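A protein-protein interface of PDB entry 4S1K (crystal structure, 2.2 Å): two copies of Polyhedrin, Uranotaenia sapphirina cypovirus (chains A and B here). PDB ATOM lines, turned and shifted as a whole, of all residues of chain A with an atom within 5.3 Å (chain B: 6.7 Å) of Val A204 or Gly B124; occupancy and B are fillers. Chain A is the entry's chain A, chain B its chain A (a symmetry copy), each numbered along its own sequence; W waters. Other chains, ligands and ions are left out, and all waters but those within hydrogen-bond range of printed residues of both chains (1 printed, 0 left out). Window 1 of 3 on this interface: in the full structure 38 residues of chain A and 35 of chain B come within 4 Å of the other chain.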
ATOM      1  N   ASN A  26      -0.033 -17.050 -13.115  1.00  0.00           N
ATOM      2  CA  ASN A  26      -1.316 -17.673 -12.758  1.00  0.00           C
ATOM      3  C   ASN A  26      -1.148 -18.922 -11.904  1.00  0.00           C
ATOM      4  O   ASN A  26      -0.231 -19.690 -12.083  1.00  0.00           O
ATOM      5  CB  ASN A  26      -2.062 -18.058 -14.035  1.00  0.00           C
ATOM      6  CG  ASN A  26      -2.714 -16.867 -14.718  1.00  0.00           C
ATOM      7  OD1 ASN A  26      -3.051 -15.896 -14.070  1.00  0.00           O
ATOM      8  ND2 ASN A  26      -2.923 -16.958 -16.021  1.00  0.00           N
ATOM      9  N   HIS A  44     -11.021 -25.369 -17.193  1.00  0.00           N
ATOM     10  CA  HIS A  44      -9.780 -24.720 -16.817  1.00  0.00           C
ATOM     11  C   HIS A  44     -10.014 -23.270 -16.487  1.00  0.00           C
ATOM     12  O   HIS A  44     -10.633 -22.536 -17.253  1.00  0.00           O
ATOM     13  CB  HIS A  44      -8.747 -24.754 -17.936  1.00  0.00           C
ATOM     14  CG  HIS A  44      -7.531 -23.911 -17.639  1.00  0.00           C
ATOM     15  ND1 HIS A  44      -7.302 -22.693 -18.238  1.00  0.00           N
ATOM     16  CD2 HIS A  44      -6.529 -24.080 -16.749  1.00  0.00           C
ATOM     17  CE1 HIS A  44      -6.187 -22.170 -17.762  1.00  0.00           C
ATOM     18  NE2 HIS A  44      -5.706 -22.987 -16.849  1.00  0.00           N
ATOM     19  N   ALA A  46      -7.811 -19.917 -14.508  1.00  0.00           N
ATOM     20  CA  ALA A  46      -6.525 -19.393 -14.059  1.00  0.00           C
ATOM     21  C   ALA A  46      -6.615 -17.961 -13.563  1.00  0.00           C
ATOM     22  O   ALA A  46      -7.400 -17.118 -14.093  1.00  0.00           O
ATOM     23  CB  ALA A  46      -5.489 -19.489 -15.169  1.00  0.00           C
ATOM     24  N   ASN A  47      -5.765 -17.668 -12.575  1.00  0.00           N
ATOM     25  CA  ASN A  47      -5.646 -16.301 -12.027  1.00  0.00           C
ATOM     26  C   ASN A  47      -4.441 -16.217 -11.124  1.00  0.00           C
ATOM     27  O   ASN A  47      -4.085 -17.235 -10.557  1.00  0.00           O
ATOM     28  CB  ASN A  47      -6.864 -15.899 -11.196  1.00  0.00           C
ATOM     29  CG  ASN A  47      -6.923 -14.434 -10.998  1.00  0.00           C
ATOM     30  OD1 ASN A  47      -6.554 -13.906  -9.953  1.00  0.00           O
ATOM     31  ND2 ASN A  47      -7.270 -13.741 -12.060  1.00  0.00           N
ATOM     32  N   ASP A 202     -10.215 -12.243 -12.103  1.00  0.00           N
ATOM     33  CA  ASP A 202     -11.260 -12.512 -13.109  1.00  0.00           C
ATOM     34  C   ASP A 202     -10.925 -11.959 -14.541  1.00  0.00           C
ATOM     35  O   ASP A 202     -11.780 -11.402 -15.237  1.00  0.00           O
ATOM     36  CB  ASP A 202     -12.621 -11.931 -12.644  1.00  0.00           C
ATOM     37  CG  ASP A 202     -12.974 -12.257 -11.168  1.00  0.00           C
ATOM     38  OD1 ASP A 202     -12.505 -13.269 -10.609  1.00  0.00           O
ATOM     39  OD2 ASP A 202     -13.757 -11.483 -10.565  1.00  0.00           O
ATOM     40  N   THR A 203      -9.685 -12.119 -14.984  1.00  0.00           N
ATOM     41  CA  THR A 203      -9.257 -11.580 -16.275  1.00  0.00           C
ATOM     42  C   THR A 203      -8.889 -12.638 -17.329  1.00  0.00           C
ATOM     43  O   THR A 203      -8.578 -12.295 -18.471  1.00  0.00           O
ATOM     44  CB  THR A 203      -8.031 -10.674 -16.071  1.00  0.00           C
ATOM     45  OG1 THR A 203      -7.112 -11.332 -15.194  1.00  0.00           O
ATOM     46  CG2 THR A 203      -8.449  -9.347 -15.428  1.00  0.00           C
ATOM     47  N   VAL A 204      -8.870 -13.904 -16.952  1.00  0.00           N
ATOM     48  CA  VAL A 204      -8.345 -14.936 -17.833  1.00  0.00           C
ATOM     49  C   VAL A 204      -9.536 -15.768 -18.320  1.00  0.00           C
ATOM     50  O   VAL A 204     -10.312 -16.196 -17.515  1.00  0.00           O
ATOM     51  CB  VAL A 204      -7.344 -15.860 -17.096  1.00  0.00           C
ATOM     52  CG1 VAL A 204      -6.860 -16.999 -17.988  1.00  0.00           C
ATOM     53  CG2 VAL A 204      -6.190 -15.066 -16.536  1.00  0.00           C
ATOM     54  N   PRO A 205      -9.671 -15.966 -19.644  1.00  0.00           N
ATOM     55  CA  PRO A 205     -10.734 -16.797 -20.199  1.00  0.00           C
ATOM     56  C   PRO A 205     -10.754 -18.176 -19.560  1.00  0.00           C
ATOM     57  O   PRO A 205      -9.706 -18.780 -19.389  1.00  0.00           O
ATOM     58  CB  PRO A 205     -10.342 -16.954 -21.684  1.00  0.00           C
ATOM     59  CG  PRO A 205      -9.250 -15.981 -21.966  1.00  0.00           C
ATOM     60  CD  PRO A 205      -8.698 -15.507 -20.668  1.00  0.00           C
ATOM     61  N   GLU A 206     -11.930 -18.658 -19.204  1.00  0.00           N
ATOM     62  CA  GLU A 206     -12.133 -20.065 -18.878  1.00  0.00           C
ATOM     63  C   GLU A 206     -12.190 -20.902 -20.157  1.00  0.00           C
ATOM     64  O   GLU A 206     -12.557 -20.379 -21.214  1.00  0.00           O
ATOM     65  CB  GLU A 206     -13.448 -20.223 -18.113  1.00  0.00           C
ATOM     66  CG  GLU A 206     -13.771 -21.654 -17.670  1.00  0.00           C
ATOM     67  CD  GLU A 206     -14.581 -22.497 -18.653  1.00  0.00           C
ATOM     68  OE1 GLU A 206     -15.260 -21.964 -19.552  1.00  0.00           O
ATOM     69  OE2 GLU A 206     -14.566 -23.737 -18.483  1.00  0.00           O
ATOM     70  N   VAL B  54     -13.167 -10.084 -21.309  1.00  0.00           N
ATOM     71  CA  VAL B  54     -12.608 -11.416 -21.485  1.00  0.00           C
ATOM     72  C   VAL B  54     -13.431 -12.177 -22.498  1.00  0.00           C
ATOM     73  O   VAL B  54     -14.619 -12.324 -22.310  1.00  0.00           O
ATOM     74  CB  VAL B  54     -12.632 -12.190 -20.162  1.00  0.00           C
ATOM     75  CG1 VAL B  54     -11.981 -13.572 -20.345  1.00  0.00           C
ATOM     76  CG2 VAL B  54     -11.962 -11.370 -19.072  1.00  0.00           C
ATOM     77  N   SER B  57     -12.013 -18.204 -27.056  1.00  0.00           N
ATOM     78  CA  SER B  57     -11.765 -18.382 -28.473  1.00  0.00           C
ATOM     79  C   SER B  57     -13.014 -18.934 -29.165  1.00  0.00           C
ATOM     80  O   SER B  57     -13.238 -18.613 -30.321  1.00  0.00           O
ATOM     81  CB  SER B  57     -10.586 -19.317 -28.683  1.00  0.00           C
ATOM     82  OG  SER B  57     -10.852 -20.515 -27.996  1.00  0.00           O
ATOM     83  N   ARG B 120      -4.419 -13.808 -26.242  1.00  0.00           N
ATOM     84  CA  ARG B 120      -3.974 -15.015 -25.589  1.00  0.00           C
ATOM     85  C   ARG B 120      -4.220 -16.149 -26.546  1.00  0.00           C
ATOM     86  O   ARG B 120      -4.875 -15.971 -27.561  1.00  0.00           O
ATOM     87  CB  ARG B 120      -4.731 -15.228 -24.290  1.00  0.00           C
ATOM     88  CG  ARG B 120      -4.443 -14.148 -23.245  1.00  0.00           C
ATOM     89  CD  ARG B 120      -5.337 -14.307 -22.025  1.00  0.00           C
ATOM     90  NE  ARG B 120      -4.845 -15.342 -21.170  1.00  0.00           N
ATOM     91  CZ  ARG B 120      -3.785 -15.224 -20.367  1.00  0.00           C
ATOM     92  NH1 ARG B 120      -3.097 -14.079 -20.307  1.00  0.00           N
ATOM     93  NH2 ARG B 120      -3.398 -16.271 -19.624  1.00  0.00           N
ATOM     94  N   GLY B 121      -3.692 -17.310 -26.227  1.00  0.00           N
ATOM     95  CA  GLY B 121      -3.815 -18.432 -27.106  1.00  0.00           C
ATOM     96  C   GLY B 121      -5.180 -19.059 -27.084  1.00  0.00           C
ATOM     97  O   GLY B 121      -6.045 -18.654 -26.313  1.00  0.00           O
ATOM     98  N   PRO B 122      -5.382 -20.070 -27.932  1.00  0.00           N
ATOM     99  CA  PRO B 122      -6.714 -20.640 -28.171  1.00  0.00           C
ATOM    100  C   PRO B 122      -7.444 -21.219 -26.959  1.00  0.00           C
ATOM    101  O   PRO B 122      -8.683 -21.365 -26.986  1.00  0.00           O
ATOM    102  CB  PRO B 122      -6.451 -21.735 -29.228  1.00  0.00           C
ATOM    103  CG  PRO B 122      -5.008 -22.002 -29.207  1.00  0.00           C
ATOM    104  CD  PRO B 122      -4.326 -20.746 -28.717  1.00  0.00           C
ATOM    105  N   THR B 123      -6.695 -21.617 -25.930  1.00  0.00           N
ATOM    106  CA  THR B 123      -7.301 -22.190 -24.722  1.00  0.00           C
ATOM    107  C   THR B 123      -7.140 -21.280 -23.485  1.00  0.00           C
ATOM    108  O   THR B 123      -7.386 -21.707 -22.355  1.00  0.00           O
ATOM    109  CB  THR B 123      -6.727 -23.578 -24.431  1.00  0.00           C
ATOM    110  OG1 THR B 123      -5.315 -23.459 -24.286  1.00  0.00           O
ATOM    111  CG2 THR B 123      -7.053 -24.554 -25.570  1.00  0.00           C
ATOM    112  N   GLY B 124      -6.713 -20.038 -23.722  1.00  0.00           N
ATOM    113  CA  GLY B 124      -6.603 -19.022 -22.678  1.00  0.00           C
ATOM    114  C   GLY B 124      -5.226 -18.847 -22.050  1.00  0.00           C
ATOM    115  O   GLY B 124      -5.093 -18.025 -21.140  1.00  0.00           O
ATOM    116  N   LEU B 125      -4.208 -19.588 -22.499  1.00  0.00           N
ATOM    117  CA  LEU B 125      -2.883 -19.456 -21.924  1.00  0.00           C
ATOM    118  C   LEU B 125      -2.174 -18.286 -22.592  1.00  0.00           C
ATOM    119  O   LEU B 125      -2.531 -17.885 -23.707  1.00  0.00           O
ATOM    120  CB  LEU B 125      -2.054 -20.748 -22.044  1.00  0.00           C
ATOM    121  CG  LEU B 125      -2.743 -22.014 -21.504  1.00  0.00           C
ATOM    122  CD1 LEU B 125      -1.933 -23.304 -21.702  1.00  0.00           C
ATOM    123  CD2 LEU B 125      -3.052 -21.817 -20.038  1.00  0.00           C
ATOM    124  N   SER B 126      -1.172 -17.735 -21.898  1.00  0.00           N
ATOM    125  CA  SER B 126      -0.368 -16.653 -22.441  1.00  0.00           C
ATOM    126  C   SER B 126       0.145 -17.089 -23.803  1.00  0.00           C
ATOM    127  O   SER B 126       0.583 -18.241 -23.950  1.00  0.00           O
ATOM    128  CB  SER B 126       0.809 -16.374 -21.521  1.00  0.00           C
ATOM    129  OG  SER B 126       0.345 -15.812 -20.341  1.00  0.00           O
ATOM    130  N   MET B 127       0.089 -16.189 -24.787  1.00  0.00           N
ATOM    131  CA  MET B 127       0.515 -16.549 -26.129  1.00  0.00           C
ATOM    132  C   MET B 127       2.015 -16.787 -26.190  1.00  0.00           C
ATOM    133  O   MET B 127       2.807 -15.981 -25.756  1.00  0.00           O
ATOM    134  CB  MET B 127       0.158 -15.480 -27.165  1.00  0.00           C
ATOM    135  CG  MET B 127       0.609 -15.850 -28.574  1.00  0.00           C
ATOM    136  SD  MET B 127      -0.245 -14.851 -29.827  1.00  0.00           S
ATOM    137  CE  MET B 127      -1.853 -15.674 -29.838  1.00  0.00           C
ATOM    138  N   GLU B 131       2.811 -22.998 -25.695  1.00  0.00           N
ATOM    139  CA  GLU B 131       1.995 -22.649 -24.537  1.00  0.00           C
ATOM    140  C   GLU B 131       2.026 -23.786 -23.532  1.00  0.00           C
ATOM    141  O   GLU B 131       2.049 -24.927 -23.906  1.00  0.00           O
ATOM    142  CB  GLU B 131       0.574 -22.303 -24.986  1.00  0.00           C
ATOM    143  CG  GLU B 131       0.596 -20.986 -25.738  1.00  0.00           C
ATOM    144  CD  GLU B 131      -0.671 -20.656 -26.512  1.00  0.00           C
ATOM    145  OE1 GLU B 131      -1.666 -21.428 -26.423  1.00  0.00           O
ATOM    146  OE2 GLU B 131      -0.651 -19.611 -27.241  1.00  0.00           O
ATOM    147  N   ASP B 136       2.201 -19.286 -17.812  1.00  0.00           N
ATOM    148  CA  ASP B 136       0.911 -18.697 -18.008  1.00  0.00           C
ATOM    149  C   ASP B 136       0.769 -17.565 -16.991  1.00  0.00           C
ATOM    150  O   ASP B 136       0.881 -17.774 -15.780  1.00  0.00           O
ATOM    151  CB  ASP B 136      -0.164 -19.758 -17.819  1.00  0.00           C
ATOM    152  CG  ASP B 136      -1.554 -19.230 -18.104  1.00  0.00           C
ATOM    153  OD1 ASP B 136      -1.708 -18.457 -19.090  1.00  0.00           O
ATOM    154  OD2 ASP B 136      -2.471 -19.577 -17.320  1.00  0.00           O
ATOM    155  N   ARG B 137       0.546 -16.363 -17.497  1.00  0.00           N
ATOM    156  CA  ARG B 137       0.560 -15.176 -16.662  1.00  0.00           C
ATOM    157  C   ARG B 137      -0.363 -14.141 -17.257  1.00  0.00           C
ATOM    158  O   ARG B 137      -0.903 -14.358 -18.330  1.00  0.00           O
ATOM    159  CB  ARG B 137       1.991 -14.630 -16.492  1.00  0.00           C
ATOM    160  CG  ARG B 137       2.831 -14.543 -17.785  1.00  0.00           C
ATOM    161  CD  ARG B 137       2.637 -13.241 -18.548  1.00  0.00           C
ATOM    162  NE  ARG B 137       2.870 -12.080 -17.692  1.00  0.00           N
ATOM    163  CZ  ARG B 137       4.060 -11.561 -17.387  1.00  0.00           C
ATOM    164  NH1 ARG B 137       5.175 -12.075 -17.870  1.00  0.00           N
ATOM    165  NH2 ARG B 137       4.137 -10.501 -16.584  1.00  0.00           N
ATOM    166  N   ILE B 138      -0.608 -13.066 -16.498  1.00  0.00           N
ATOM    167  CA  ILE B 138      -1.320 -11.910 -16.997  1.00  0.00           C
ATOM    168  C   ILE B 138      -0.404 -10.710 -17.091  1.00  0.00           C
ATOM    169  O   ILE B 138       0.754 -10.707 -16.660  1.00  0.00           O
ATOM    170  CB  ILE B 138      -2.559 -11.564 -16.172  1.00  0.00           C
ATOM    171  CG1 ILE B 138      -2.178 -10.921 -14.842  1.00  0.00           C
ATOM    172  CG2 ILE B 138      -3.434 -12.808 -15.993  1.00  0.00           C
ATOM    173  CD1 ILE B 138      -3.378 -10.459 -14.043  1.00  0.00           C
ATOM    174  N   VAL B 172      -7.520 -17.324 -31.191  1.00  0.00           N
ATOM    175  CA  VAL B 172      -6.972 -16.659 -30.015  1.00  0.00           C
ATOM    176  C   VAL B 172      -8.118 -16.420 -29.051  1.00  0.00           C
ATOM    177  O   VAL B 172      -9.283 -16.497 -29.416  1.00  0.00           O
ATOM    178  CB  VAL B 172      -6.296 -15.333 -30.401  1.00  0.00           C
ATOM    179  CG1 VAL B 172      -5.188 -15.573 -31.399  1.00  0.00           C
ATOM    180  CG2 VAL B 172      -7.293 -14.332 -30.966  1.00  0.00           C
ATOM    181  N   SER B 173      -7.772 -16.169 -27.802  1.00  0.00           N
ATOM    182  CA  SER B 173      -8.680 -15.585 -26.858  1.00  0.00           C
ATOM    183  C   SER B 173      -8.166 -14.207 -26.488  1.00  0.00           C
ATOM    184  O   SER B 173      -7.058 -13.791 -26.875  1.00  0.00           O
ATOM    185  CB  SER B 173      -8.821 -16.478 -25.637  1.00  0.00           C
ATOM    186  OG  SER B 173      -7.568 -16.810 -25.105  1.00  0.00           O
ATOM    187  N   ILE B 174      -8.991 -13.487 -25.740  1.00  0.00           N
ATOM    188  CA  ILE B 174      -8.729 -12.099 -25.446  1.00  0.00           C
ATOM    189  C   ILE B 174      -8.922 -11.797 -24.004  1.00  0.00           C
ATOM    190  O   ILE B 174      -9.894 -12.213 -23.411  1.00  0.00           O
ATOM    191  CB  ILE B 174      -9.730 -11.182 -26.168  1.00  0.00           C
ATOM    192  CG1 ILE B 174      -9.568 -11.325 -27.688  1.00  0.00           C
ATOM    193  CG2 ILE B 174      -9.542  -9.727 -25.675  1.00  0.00           C
ATOM    194  CD1 ILE B 174     -10.558 -10.490 -28.472  1.00  0.00           C
ATOM    195  N   ALA B 175      -8.030 -10.994 -23.466  1.00  0.00           N
ATOM    196  CA  ALA B 175      -8.230 -10.457 -22.162  1.00  0.00           C
ATOM    197  C   ALA B 175      -7.823  -8.994 -22.213  1.00  0.00           C
ATOM    198  O   ALA B 175      -6.665  -8.654 -22.486  1.00  0.00           O
ATOM    199  CB  ALA B 175      -7.397 -11.257 -21.166  1.00  0.00           C
HETATM  200  O   HOH W   1      -8.602 -20.854 -19.992  1.00  0.00           O
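Of the printed residues of chain B, Asn A26 touches Arg B120 (3.7 Å), Asp B136 (2.9 Å), Arg B137 (3.8 Å) and Ile B138 (3.7 Å).
Of chain B, only Val B54, Arg B120, Gly B124 and Ile B138 come within 4 Å of Val A204.
Of the printed residues of chain B, Pro A205 touches Val B54, Arg B120 and Ser B173.
Of chain A, only Val A204 (3.8 Å) comes within 4 Å of Gly B124.
The nearest printed residue of chain A that does not touch Asp B136 is His A44 (4.6 Å).
N of Asn A26 sits at hydrogen-bond distance from O of Asp B136 (2.9 Å).
No position is printed for both chains.
Of the 16 pairs that touch across the chains among the printed residues, none has its exchanged pair printed and touching as well.
Among the printed residues, merely in contact across the chains: Thr A203 with Ala B175, Pro A205 with Val B54, Thr A203 with Val B54, Val A204 with Ile B138, Pro A205 with Ser B173, Asn A26 with Ile B138, Asn A26 with Arg B120, Ala A46 with Asp B136, Val A204 with Gly B124, Asn A26 with Arg B137, Pro A205 with Arg B120, Asp A202 with Val B54, Val A204 with Val B54, His A44 with Leu B125 and Val A204 with Arg B120.
Water W1 lies within hydrogen-bond range of the backbone carbonyl oxygen of Pro A205, the backbone carbonyl oxygen of Thr B123 and a ring nitrogen (ND1) of His A44.
Of the 9 printed residues of chain A, 7 touch a printed residue of chain B.
Hydrophobic or aromatic side chains of chain A within 4 Å of the printed part of chain B: His A44, Ala A46, Val A204 and Pro A205.
Of the 18 printed residues of chain B, 9 touch a printed residue of chain A.
Hydrophobic or aromatic side chains of chain B within 4 Å of the printed part of chain A: Val B54, Leu B125, Ile B138 and Ala B175.
N of Asp A202 sits close to ND2 of Asn A47, at 3.3 Å.
The side-chain carboxylate (OD1) of Asp B136 lies within salt-bridge range of the guanidinium group (NH2) of Arg B120 (2.8 Å).
The guanidinium group (NH1) of Arg B120 lies within hydrogen-bond range of the backbone carbonyl oxygen (O) of Arg B137.
The backbone NH (N) of Arg B120 is in hydrogen-bond range of the backbone carbonyl oxygen (O) of Ser B173, at 2.7 Å.
O of Gly B121 sits at hydrogen-bond distance from OG of Ser B173 (2.7 Å).
N of Ser B126 lies within hydrogen-bond range of OD1 of Asp B136 (2.9 Å).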
